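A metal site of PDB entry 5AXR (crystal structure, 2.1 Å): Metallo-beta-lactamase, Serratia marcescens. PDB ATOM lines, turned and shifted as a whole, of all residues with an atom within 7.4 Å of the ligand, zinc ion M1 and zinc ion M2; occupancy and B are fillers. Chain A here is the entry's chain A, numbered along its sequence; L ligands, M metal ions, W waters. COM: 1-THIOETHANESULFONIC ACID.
Three residues have an atom within 4 Å of zinc ion M1: Asp 76, His 77 and His 215. The nearest printed residue that does not touch zinc ion M1 is Ile 26 (4.3 Å).
Water W1 lies within hydrogen-bond range of the side-chain hydroxyl of Thr 177 and an oxygen (O3S) of the ligand.
NE2 of Gln 113 lies within hydrogen-bond range of O1S of the ligand (2.7 Å).
Within 4 Å of zinc ion M2: His 72, His 74 and His 150.
Zinc ion M2 is bound by a sulfur (S1) of the ligand (2.0 Å), a ring nitrogen (ND1) of His 74 (2.0 Å), a ring nitrogen (NE2) of His 150 (2.1 Å) and a ring nitrogen (NE2) of His 72 (2.1 Å). Zinc ion M2 has four donor atoms within binding distance.
Merely in contact with the ligand: Val 179 (3.3 Å), Trp 5 (3.4 Å) and Leu 117 (3.7 Å). Hydrophobic or aromatic side chains that line the ligand: Trp 5, Leu 117, His 150, Val 179 and His 215. Ten residues have an atom within 4 Å of the ligand: Trp 5, His 72, His 74, Asp 76, His 77, Gln 113, Leu 117, His 150, Val 179 and His 215. Along chain A the residues within 4 Å of the ligand span positions 5 to 215.
Zinc ion M1 is bound by OD2 of Asp 76 (2.0 Å). Zinc ion M1 is bound by NE2 of His 77 (2.1 Å). NE2 of His 215 is bound to zinc ion M1 (2.1 Å). A sulfur (S1) of the ligand is bound to zinc ion M1 (2.3 Å). Zinc ion M1 has four donor atoms within binding distance.
NE2 of His 74 sits at hydrogen-bond distance from OD1 of Asp 111 (2.8 Å). ND1 of His 72 lies within hydrogen-bond range of OD1 of Asp 174, at 2.6 Å. The backbone carbonyl oxygen of Thr 177 lies within hydrogen-bond range of a ring nitrogen (ND1) of His 150 (2.8 Å). The backbone NH (N) of Gln 113 is in hydrogen-bond range of the side-chain carboxylate (OD1) of Asp 111 (2.8 Å). OE1 of Gln 113 lies close to O of Val 179.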
ATOM      1  N   TRP A   5     -15.556 -27.343  14.601  1.00  0.00           N
ATOM      2  CA  TRP A   5     -14.474 -27.864  15.424  1.00  0.00           C
ATOM      3  C   TRP A   5     -14.628 -29.349  15.746  1.00  0.00           C
ATOM      4  O   TRP A   5     -13.638 -30.026  16.046  1.00  0.00           O
ATOM      5  CB  TRP A   5     -14.376 -27.021  16.701  1.00  0.00           C
ATOM      6  CG  TRP A   5     -13.978 -25.582  16.448  1.00  0.00           C
ATOM      7  CD1 TRP A   5     -13.429 -25.065  15.316  1.00  0.00           C
ATOM      8  CD2 TRP A   5     -14.087 -24.494  17.370  1.00  0.00           C
ATOM      9  NE1 TRP A   5     -13.176 -23.726  15.473  1.00  0.00           N
ATOM     10  CE2 TRP A   5     -13.548 -23.349  16.733  1.00  0.00           C
ATOM     11  CE3 TRP A   5     -14.532 -24.381  18.682  1.00  0.00           C
ATOM     12  CZ2 TRP A   5     -13.428 -22.117  17.375  1.00  0.00           C
ATOM     13  CZ3 TRP A   5     -14.461 -23.141  19.303  1.00  0.00           C
ATOM     14  CH2 TRP A   5     -13.927 -22.031  18.641  1.00  0.00           C
ATOM     15  N   GLY A  25     -12.271 -28.977  11.561  1.00  0.00           N
ATOM     16  CA  GLY A  25     -11.896 -27.609  11.992  1.00  0.00           C
ATOM     17  C   GLY A  25     -10.716 -27.446  12.942  1.00  0.00           C
ATOM     18  O   GLY A  25     -10.278 -26.324  13.162  1.00  0.00           O
ATOM     19  N   ILE A  26     -10.309 -28.539  13.602  1.00  0.00           N
ATOM     20  CA  ILE A  26      -9.210 -28.544  14.579  1.00  0.00           C
ATOM     21  C   ILE A  26      -8.205 -29.679  14.271  1.00  0.00           C
ATOM     22  O   ILE A  26      -8.587 -30.852  14.074  1.00  0.00           O
ATOM     23  CB  ILE A  26      -9.724 -28.721  16.027  1.00  0.00           C
ATOM     24  CG1 ILE A  26     -10.695 -27.596  16.435  1.00  0.00           C
ATOM     25  CG2 ILE A  26      -8.569 -28.752  17.013  1.00  0.00           C
ATOM     26  CD1 ILE A  26     -10.018 -26.247  16.610  1.00  0.00           C
ATOM     27  N   HIS A  72      -2.185 -26.005  23.570  1.00  0.00           N
ATOM     28  CA  HIS A  72      -2.701 -25.206  24.662  1.00  0.00           C
ATOM     29  C   HIS A  72      -4.075 -25.664  25.108  1.00  0.00           C
ATOM     30  O   HIS A  72      -4.829 -26.366  24.387  1.00  0.00           O
ATOM     31  CB  HIS A  72      -2.702 -23.703  24.284  1.00  0.00           C
ATOM     32  CG  HIS A  72      -3.734 -23.319  23.272  1.00  0.00           C
ATOM     33  ND1 HIS A  72      -3.561 -23.494  21.913  1.00  0.00           N
ATOM     34  CD2 HIS A  72      -4.977 -22.796  23.415  1.00  0.00           C
ATOM     35  CE1 HIS A  72      -4.627 -23.057  21.270  1.00  0.00           C
ATOM     36  NE2 HIS A  72      -5.506 -22.641  22.155  1.00  0.00           N
ATOM     37  N   SER A  73      -4.439 -25.169  26.284  1.00  0.00           N
ATOM     38  CA  SER A  73      -5.540 -25.724  27.036  1.00  0.00           C
ATOM     39  C   SER A  73      -6.833 -24.949  26.828  1.00  0.00           C
ATOM     40  O   SER A  73      -7.430 -24.497  27.806  1.00  0.00           O
ATOM     41  CB  SER A  73      -5.172 -25.727  28.531  1.00  0.00           C
ATOM     42  OG  SER A  73      -4.756 -24.443  28.967  1.00  0.00           O
ATOM     43  N   HIS A  74      -7.219 -24.702  25.587  1.00  0.00           N
ATOM     44  CA  HIS A  74      -8.565 -24.249  25.291  1.00  0.00           C
ATOM     45  C   HIS A  74      -9.370 -25.450  24.849  1.00  0.00           C
ATOM     46  O   HIS A  74      -8.814 -26.414  24.318  1.00  0.00           O
ATOM     47  CB  HIS A  74      -8.576 -23.199  24.189  1.00  0.00           C
ATOM     48  CG  HIS A  74      -8.112 -21.859  24.634  1.00  0.00           C
ATOM     49  ND1 HIS A  74      -7.536 -20.962  23.766  1.00  0.00           N
ATOM     50  CD2 HIS A  74      -7.989 -21.321  25.870  1.00  0.00           C
ATOM     51  CE1 HIS A  74      -7.223 -19.862  24.430  1.00  0.00           C
ATOM     52  NE2 HIS A  74      -7.426 -20.081  25.712  1.00  0.00           N
ATOM     53  N   GLU A  75     -10.702 -25.320  24.960  1.00  0.00           N
ATOM     54  CA  GLU A  75     -11.621 -26.443  24.797  1.00  0.00           C
ATOM     55  C   GLU A  75     -11.608 -27.019  23.400  1.00  0.00           C
ATOM     56  O   GLU A  75     -11.951 -28.177  23.192  1.00  0.00           O
ATOM     57  CB  GLU A  75     -13.058 -26.030  25.102  1.00  0.00           C
ATOM     58  CG  GLU A  75     -13.963 -27.244  25.340  1.00  0.00           C
ATOM     59  CD  GLU A  75     -14.689 -27.806  24.106  1.00  0.00           C
ATOM     60  OE1 GLU A  75     -14.971 -29.044  24.085  1.00  0.00           O
ATOM     61  OE2 GLU A  75     -15.068 -27.022  23.195  1.00  0.00           O
ATOM     62  N   ASP A  76     -11.363 -26.150  22.420  1.00  0.00           N
ATOM     63  CA  ASP A  76     -11.368 -26.609  21.047  1.00  0.00           C
ATOM     64  C   ASP A  76     -10.163 -27.492  20.687  1.00  0.00           C
ATOM     65  O   ASP A  76     -10.257 -28.246  19.727  1.00  0.00           O
ATOM     66  CB  ASP A  76     -11.588 -25.454  20.076  1.00  0.00           C
ATOM     67  CG  ASP A  76     -10.503 -24.408  20.138  1.00  0.00           C
ATOM     68  OD1 ASP A  76      -9.946 -24.135  21.215  1.00  0.00           O
ATOM     69  OD2 ASP A  76     -10.263 -23.819  19.082  1.00  0.00           O
ATOM     70  N   HIS A  77      -9.089 -27.455  21.486  1.00  0.00           N
ATOM     71  CA  HIS A  77      -7.895 -28.281  21.238  1.00  0.00           C
ATOM     72  C   HIS A  77      -7.716 -29.369  22.288  1.00  0.00           C
ATOM     73  O   HIS A  77      -7.124 -30.417  22.007  1.00  0.00           O
ATOM     74  CB  HIS A  77      -6.620 -27.445  21.208  1.00  0.00           C
ATOM     75  CG  HIS A  77      -6.701 -26.270  20.296  1.00  0.00           C
ATOM     76  ND1 HIS A  77      -6.530 -26.386  18.939  1.00  0.00           N
ATOM     77  CD2 HIS A  77      -7.117 -24.998  20.522  1.00  0.00           C
ATOM     78  CE1 HIS A  77      -6.852 -25.239  18.361  1.00  0.00           C
ATOM     79  NE2 HIS A  77      -7.150 -24.365  19.309  1.00  0.00           N
ATOM     80  N   ASP A 111      -6.199 -16.332  31.600  1.00  0.00           N
ATOM     81  CA  ASP A 111      -6.271 -16.835  30.226  1.00  0.00           C
ATOM     82  C   ASP A 111      -7.105 -15.872  29.408  1.00  0.00           C
ATOM     83  O   ASP A 111      -8.232 -15.562  29.791  1.00  0.00           O
ATOM     84  CB  ASP A 111      -6.924 -18.216  30.239  1.00  0.00           C
ATOM     85  CG  ASP A 111      -6.860 -18.912  28.881  1.00  0.00           C
ATOM     86  OD1 ASP A 111      -7.341 -18.336  27.879  1.00  0.00           O
ATOM     87  OD2 ASP A 111      -6.381 -20.071  28.855  1.00  0.00           O
ATOM     88  N   GLN A 113      -9.070 -16.278  27.189  1.00  0.00           N
ATOM     89  CA  GLN A 113     -10.403 -16.821  26.945  1.00  0.00           C
ATOM     90  C   GLN A 113     -10.966 -17.554  28.147  1.00  0.00           C
ATOM     91  O   GLN A 113     -11.835 -18.400  27.977  1.00  0.00           O
ATOM     92  CB  GLN A 113     -10.381 -17.752  25.721  1.00  0.00           C
ATOM     93  CG  GLN A 113     -11.161 -17.184  24.550  1.00  0.00           C
ATOM     94  CD  GLN A 113     -10.398 -17.223  23.258  1.00  0.00           C
ATOM     95  OE1 GLN A 113      -9.175 -17.321  23.236  1.00  0.00           O
ATOM     96  NE2 GLN A 113     -11.116 -17.136  22.148  1.00  0.00           N
ATOM     97  N   SER A 116     -14.867 -17.027  27.954  1.00  0.00           N
ATOM     98  CA  SER A 116     -15.257 -17.003  26.535  1.00  0.00           C
ATOM     99  C   SER A 116     -15.422 -18.382  25.932  1.00  0.00           C
ATOM    100  O   SER A 116     -16.177 -18.567  24.983  1.00  0.00           O
ATOM    101  CB  SER A 116     -14.216 -16.209  25.718  1.00  0.00           C
ATOM    102  OG  SER A 116     -14.222 -16.609  24.347  1.00  0.00           O
ATOM    103  N   LEU A 117     -14.636 -19.337  26.417  1.00  0.00           N
ATOM    104  CA  LEU A 117     -14.852 -20.748  26.125  1.00  0.00           C
ATOM    105  C   LEU A 117     -15.284 -21.436  27.420  1.00  0.00           C
ATOM    106  O   LEU A 117     -14.872 -21.043  28.510  1.00  0.00           O
ATOM    107  CB  LEU A 117     -13.571 -21.382  25.552  1.00  0.00           C
ATOM    108  CG  LEU A 117     -12.993 -20.757  24.269  1.00  0.00           C
ATOM    109  CD1 LEU A 117     -11.587 -21.282  24.001  1.00  0.00           C
ATOM    110  CD2 LEU A 117     -13.870 -21.011  23.064  1.00  0.00           C
ATOM    111  N   HIS A 150      -0.950 -16.681  23.762  1.00  0.00           N
ATOM    112  CA  HIS A 150      -2.336 -16.990  23.437  1.00  0.00           C
ATOM    113  C   HIS A 150      -2.929 -17.709  24.653  1.00  0.00           C
ATOM    114  O   HIS A 150      -4.097 -17.520  24.964  1.00  0.00           O
ATOM    115  CB  HIS A 150      -2.420 -17.838  22.176  1.00  0.00           C
ATOM    116  CG  HIS A 150      -3.781 -18.361  21.852  1.00  0.00           C
ATOM    117  ND1 HIS A 150      -4.639 -17.720  20.988  1.00  0.00           N
ATOM    118  CD2 HIS A 150      -4.393 -19.532  22.186  1.00  0.00           C
ATOM    119  CE1 HIS A 150      -5.727 -18.455  20.816  1.00  0.00           C
ATOM    120  NE2 HIS A 150      -5.612 -19.541  21.566  1.00  0.00           N
ATOM    121  N   THR A 151      -2.107 -18.514  25.299  1.00  0.00           N
ATOM    122  CA  THR A 151      -2.235 -18.924  26.701  1.00  0.00           C
ATOM    123  C   THR A 151      -0.824 -18.876  27.266  1.00  0.00           C
ATOM    124  O   THR A 151       0.148 -18.829  26.502  1.00  0.00           O
ATOM    125  CB  THR A 151      -2.708 -20.401  26.886  1.00  0.00           C
ATOM    126  OG1 THR A 151      -1.703 -21.307  26.398  1.00  0.00           O
ATOM    127  CG2 THR A 151      -3.991 -20.675  26.163  1.00  0.00           C
ATOM    128  N   ASP A 174       1.425 -24.200  17.738  1.00  0.00           N
ATOM    129  CA  ASP A 174       0.424 -23.633  18.618  1.00  0.00           C
ATOM    130  C   ASP A 174      -0.071 -22.295  18.091  1.00  0.00           C
ATOM    131  O   ASP A 174       0.571 -21.649  17.242  1.00  0.00           O
ATOM    132  CB  ASP A 174       1.011 -23.473  20.011  1.00  0.00           C
ATOM    133  CG  ASP A 174      -0.040 -23.150  21.043  1.00  0.00           C
ATOM    134  OD1 ASP A 174      -1.227 -23.462  20.793  1.00  0.00           O
ATOM    135  OD2 ASP A 174       0.316 -22.525  22.065  1.00  0.00           O
ATOM    136  N   SER A 175      -1.278 -21.926  18.531  1.00  0.00           N
ATOM    137  CA  SER A 175      -1.935 -20.678  18.108  1.00  0.00           C
ATOM    138  C   SER A 175      -1.174 -19.461  18.630  1.00  0.00           C
ATOM    139  O   SER A 175      -0.781 -19.421  19.793  1.00  0.00           O
ATOM    140  CB  SER A 175      -3.368 -20.615  18.668  1.00  0.00           C
ATOM    141  OG  SER A 175      -4.144 -21.714  18.237  1.00  0.00           O
ATOM    142  N   THR A 177      -2.449 -16.257  18.148  1.00  0.00           N
ATOM    143  CA  THR A 177      -3.481 -15.268  17.851  1.00  0.00           C
ATOM    144  C   THR A 177      -3.909 -14.478  19.104  1.00  0.00           C
ATOM    145  O   THR A 177      -4.177 -15.049  20.161  1.00  0.00           O
ATOM    146  CB  THR A 177      -4.718 -15.978  17.283  1.00  0.00           C
ATOM    147  OG1 THR A 177      -5.013 -17.129  18.098  1.00  0.00           O
ATOM    148  CG2 THR A 177      -4.438 -16.408  15.852  1.00  0.00           C
ATOM    149  N   ALA A 178      -3.865 -13.152  18.986  1.00  0.00           N
ATOM    150  CA  ALA A 178      -4.400 -12.257  20.014  1.00  0.00           C
ATOM    151  C   ALA A 178      -5.935 -12.253  19.959  1.00  0.00           C
ATOM    152  O   ALA A 178      -6.520 -11.331  19.392  1.00  0.00           O
ATOM    153  CB  ALA A 178      -3.874 -10.847  19.789  1.00  0.00           C
ATOM    154  N   VAL A 179      -6.552 -13.307  20.484  1.00  0.00           N
ATOM    155  CA  VAL A 179      -7.996 -13.404  20.570  1.00  0.00           C
ATOM    156  C   VAL A 179      -8.384 -13.714  22.006  1.00  0.00           C
ATOM    157  O   VAL A 179      -7.594 -14.270  22.765  1.00  0.00           O
ATOM    158  CB  VAL A 179      -8.574 -14.505  19.626  1.00  0.00           C
ATOM    159  CG1 VAL A 179      -8.394 -14.111  18.175  1.00  0.00           C
ATOM    160  CG2 VAL A 179      -7.944 -15.861  19.886  1.00  0.00           C
ATOM    161  N   SER A 180      -9.603 -13.325  22.367  1.00  0.00           N
ATOM    162  CA  SER A 180     -10.026 -13.385  23.766  1.00  0.00           C
ATOM    163  C   SER A 180     -11.543 -13.306  23.885  1.00  0.00           C
ATOM    164  O   SER A 180     -12.251 -12.960  22.921  1.00  0.00           O
ATOM    165  CB  SER A 180      -9.422 -12.206  24.521  1.00  0.00           C
ATOM    166  OG  SER A 180      -9.912 -10.979  24.021  1.00  0.00           O
ATOM    167  N   ALA A 181     -12.033 -13.496  25.101  1.00  0.00           N
ATOM    168  CA  ALA A 181     -13.322 -12.934  25.517  1.00  0.00           C
ATOM    169  C   ALA A 181     -13.459 -11.460  25.138  1.00  0.00           C
ATOM    170  O   ALA A 181     -12.469 -10.720  25.132  1.00  0.00           O
ATOM    171  CB  ALA A 181     -13.504 -13.096  27.021  1.00  0.00           C
ATOM    172  N   ALA A 214      -2.599 -25.431  14.616  1.00  0.00           N
ATOM    173  CA  ALA A 214      -3.631 -25.967  15.510  1.00  0.00           C
ATOM    174  C   ALA A 214      -5.011 -25.725  14.923  1.00  0.00           C
ATOM    175  O   ALA A 214      -5.823 -26.649  14.852  1.00  0.00           O
ATOM    176  CB  ALA A 214      -3.518 -25.355  16.901  1.00  0.00           C
ATOM    177  N   HIS A 215      -5.207 -24.532  14.349  1.00  0.00           N
ATOM    178  CA  HIS A 215      -6.292 -24.314  13.384  1.00  0.00           C
ATOM    179  C   HIS A 215      -5.779 -24.558  11.977  1.00  0.00           C
ATOM    180  O   HIS A 215      -5.072 -23.722  11.440  1.00  0.00           O
ATOM    181  CB  HIS A 215      -6.893 -22.908  13.538  1.00  0.00           C
ATOM    182  CG  HIS A 215      -7.731 -22.746  14.758  1.00  0.00           C
ATOM    183  ND1 HIS A 215      -9.100 -22.906  14.733  1.00  0.00           N
ATOM    184  CD2 HIS A 215      -7.388 -22.635  16.075  1.00  0.00           C
ATOM    185  CE1 HIS A 215      -9.566 -22.890  15.969  1.00  0.00           C
ATOM    186  NE2 HIS A 215      -8.551 -22.729  16.802  1.00  0.00           N
ATOM    187  N   GLU A 217      -6.534 -24.514   8.792  1.00  0.00           N
ATOM    188  CA  GLU A 217      -6.604 -23.561   7.682  1.00  0.00           C
ATOM    189  C   GLU A 217      -5.615 -22.400   7.822  1.00  0.00           C
ATOM    190  O   GLU A 217      -5.293 -21.715   6.866  1.00  0.00           O
ATOM    191  CB  GLU A 217      -8.052 -23.077   7.506  1.00  0.00           C
ATOM    192  CG  GLU A 217      -8.559 -22.034   8.493  1.00  0.00           C
ATOM    193  CD  GLU A 217      -8.796 -22.522   9.922  1.00  0.00           C
ATOM    194  OE1 GLU A 217      -8.892 -23.728  10.186  1.00  0.00           O
ATOM    195  OE2 GLU A 217      -8.899 -21.664  10.799  1.00  0.00           O
ATOM    196  N   ARG A 252      -2.078  -9.509  13.295  1.00  0.00           N
ATOM    197  CA  ARG A 252      -3.308  -9.597  14.081  1.00  0.00           C
ATOM    198  C   ARG A 252      -3.221  -8.861  15.429  1.00  0.00           C
ATOM    199  O   ARG A 252      -4.131  -8.151  15.807  1.00  0.00           O
ATOM    200  CB  ARG A 252      -3.752 -11.034  14.289  1.00  0.00           C
ATOM    201  CG  ARG A 252      -5.029 -11.137  15.116  1.00  0.00           C
ATOM    202  CD  ARG A 252      -5.349 -12.575  15.440  1.00  0.00           C
ATOM    203  NE  ARG A 252      -5.864 -13.303  14.280  1.00  0.00           N
ATOM    204  CZ  ARG A 252      -7.156 -13.436  14.000  1.00  0.00           C
ATOM    205  NH1 ARG A 252      -8.082 -12.869  14.758  1.00  0.00           N
ATOM    206  NH2 ARG A 252      -7.522 -14.160  12.954  1.00  0.00           N
HETATM  207  C1  COM L   1      -9.828 -20.726  20.738  1.00  0.00           C
HETATM  208  C2  COM L   1     -10.841 -20.678  19.578  1.00  0.00           C
HETATM  209  S1  COM L   1      -8.118 -20.985  20.186  1.00  0.00           S
HETATM  210  S2  COM L   1     -10.777 -19.276  18.673  1.00  0.00           S
HETATM  211  O1S COM L   1     -10.429 -18.021  19.671  1.00  0.00           O
HETATM  212  O2S COM L   1     -12.038 -19.069  18.050  1.00  0.00           O
HETATM  213  O3S COM L   1      -9.748 -19.387  17.663  1.00  0.00           O
HETATM  214 ZN    ZN M   1      -8.504 -22.878  18.906  1.00  0.00          ZN
HETATM  215 ZN    ZN M   2      -6.927 -21.138  21.821  1.00  0.00          ZN
HETATM  216  O   HOH W   1      -7.123 -18.607  17.129  1.00  0.00           O
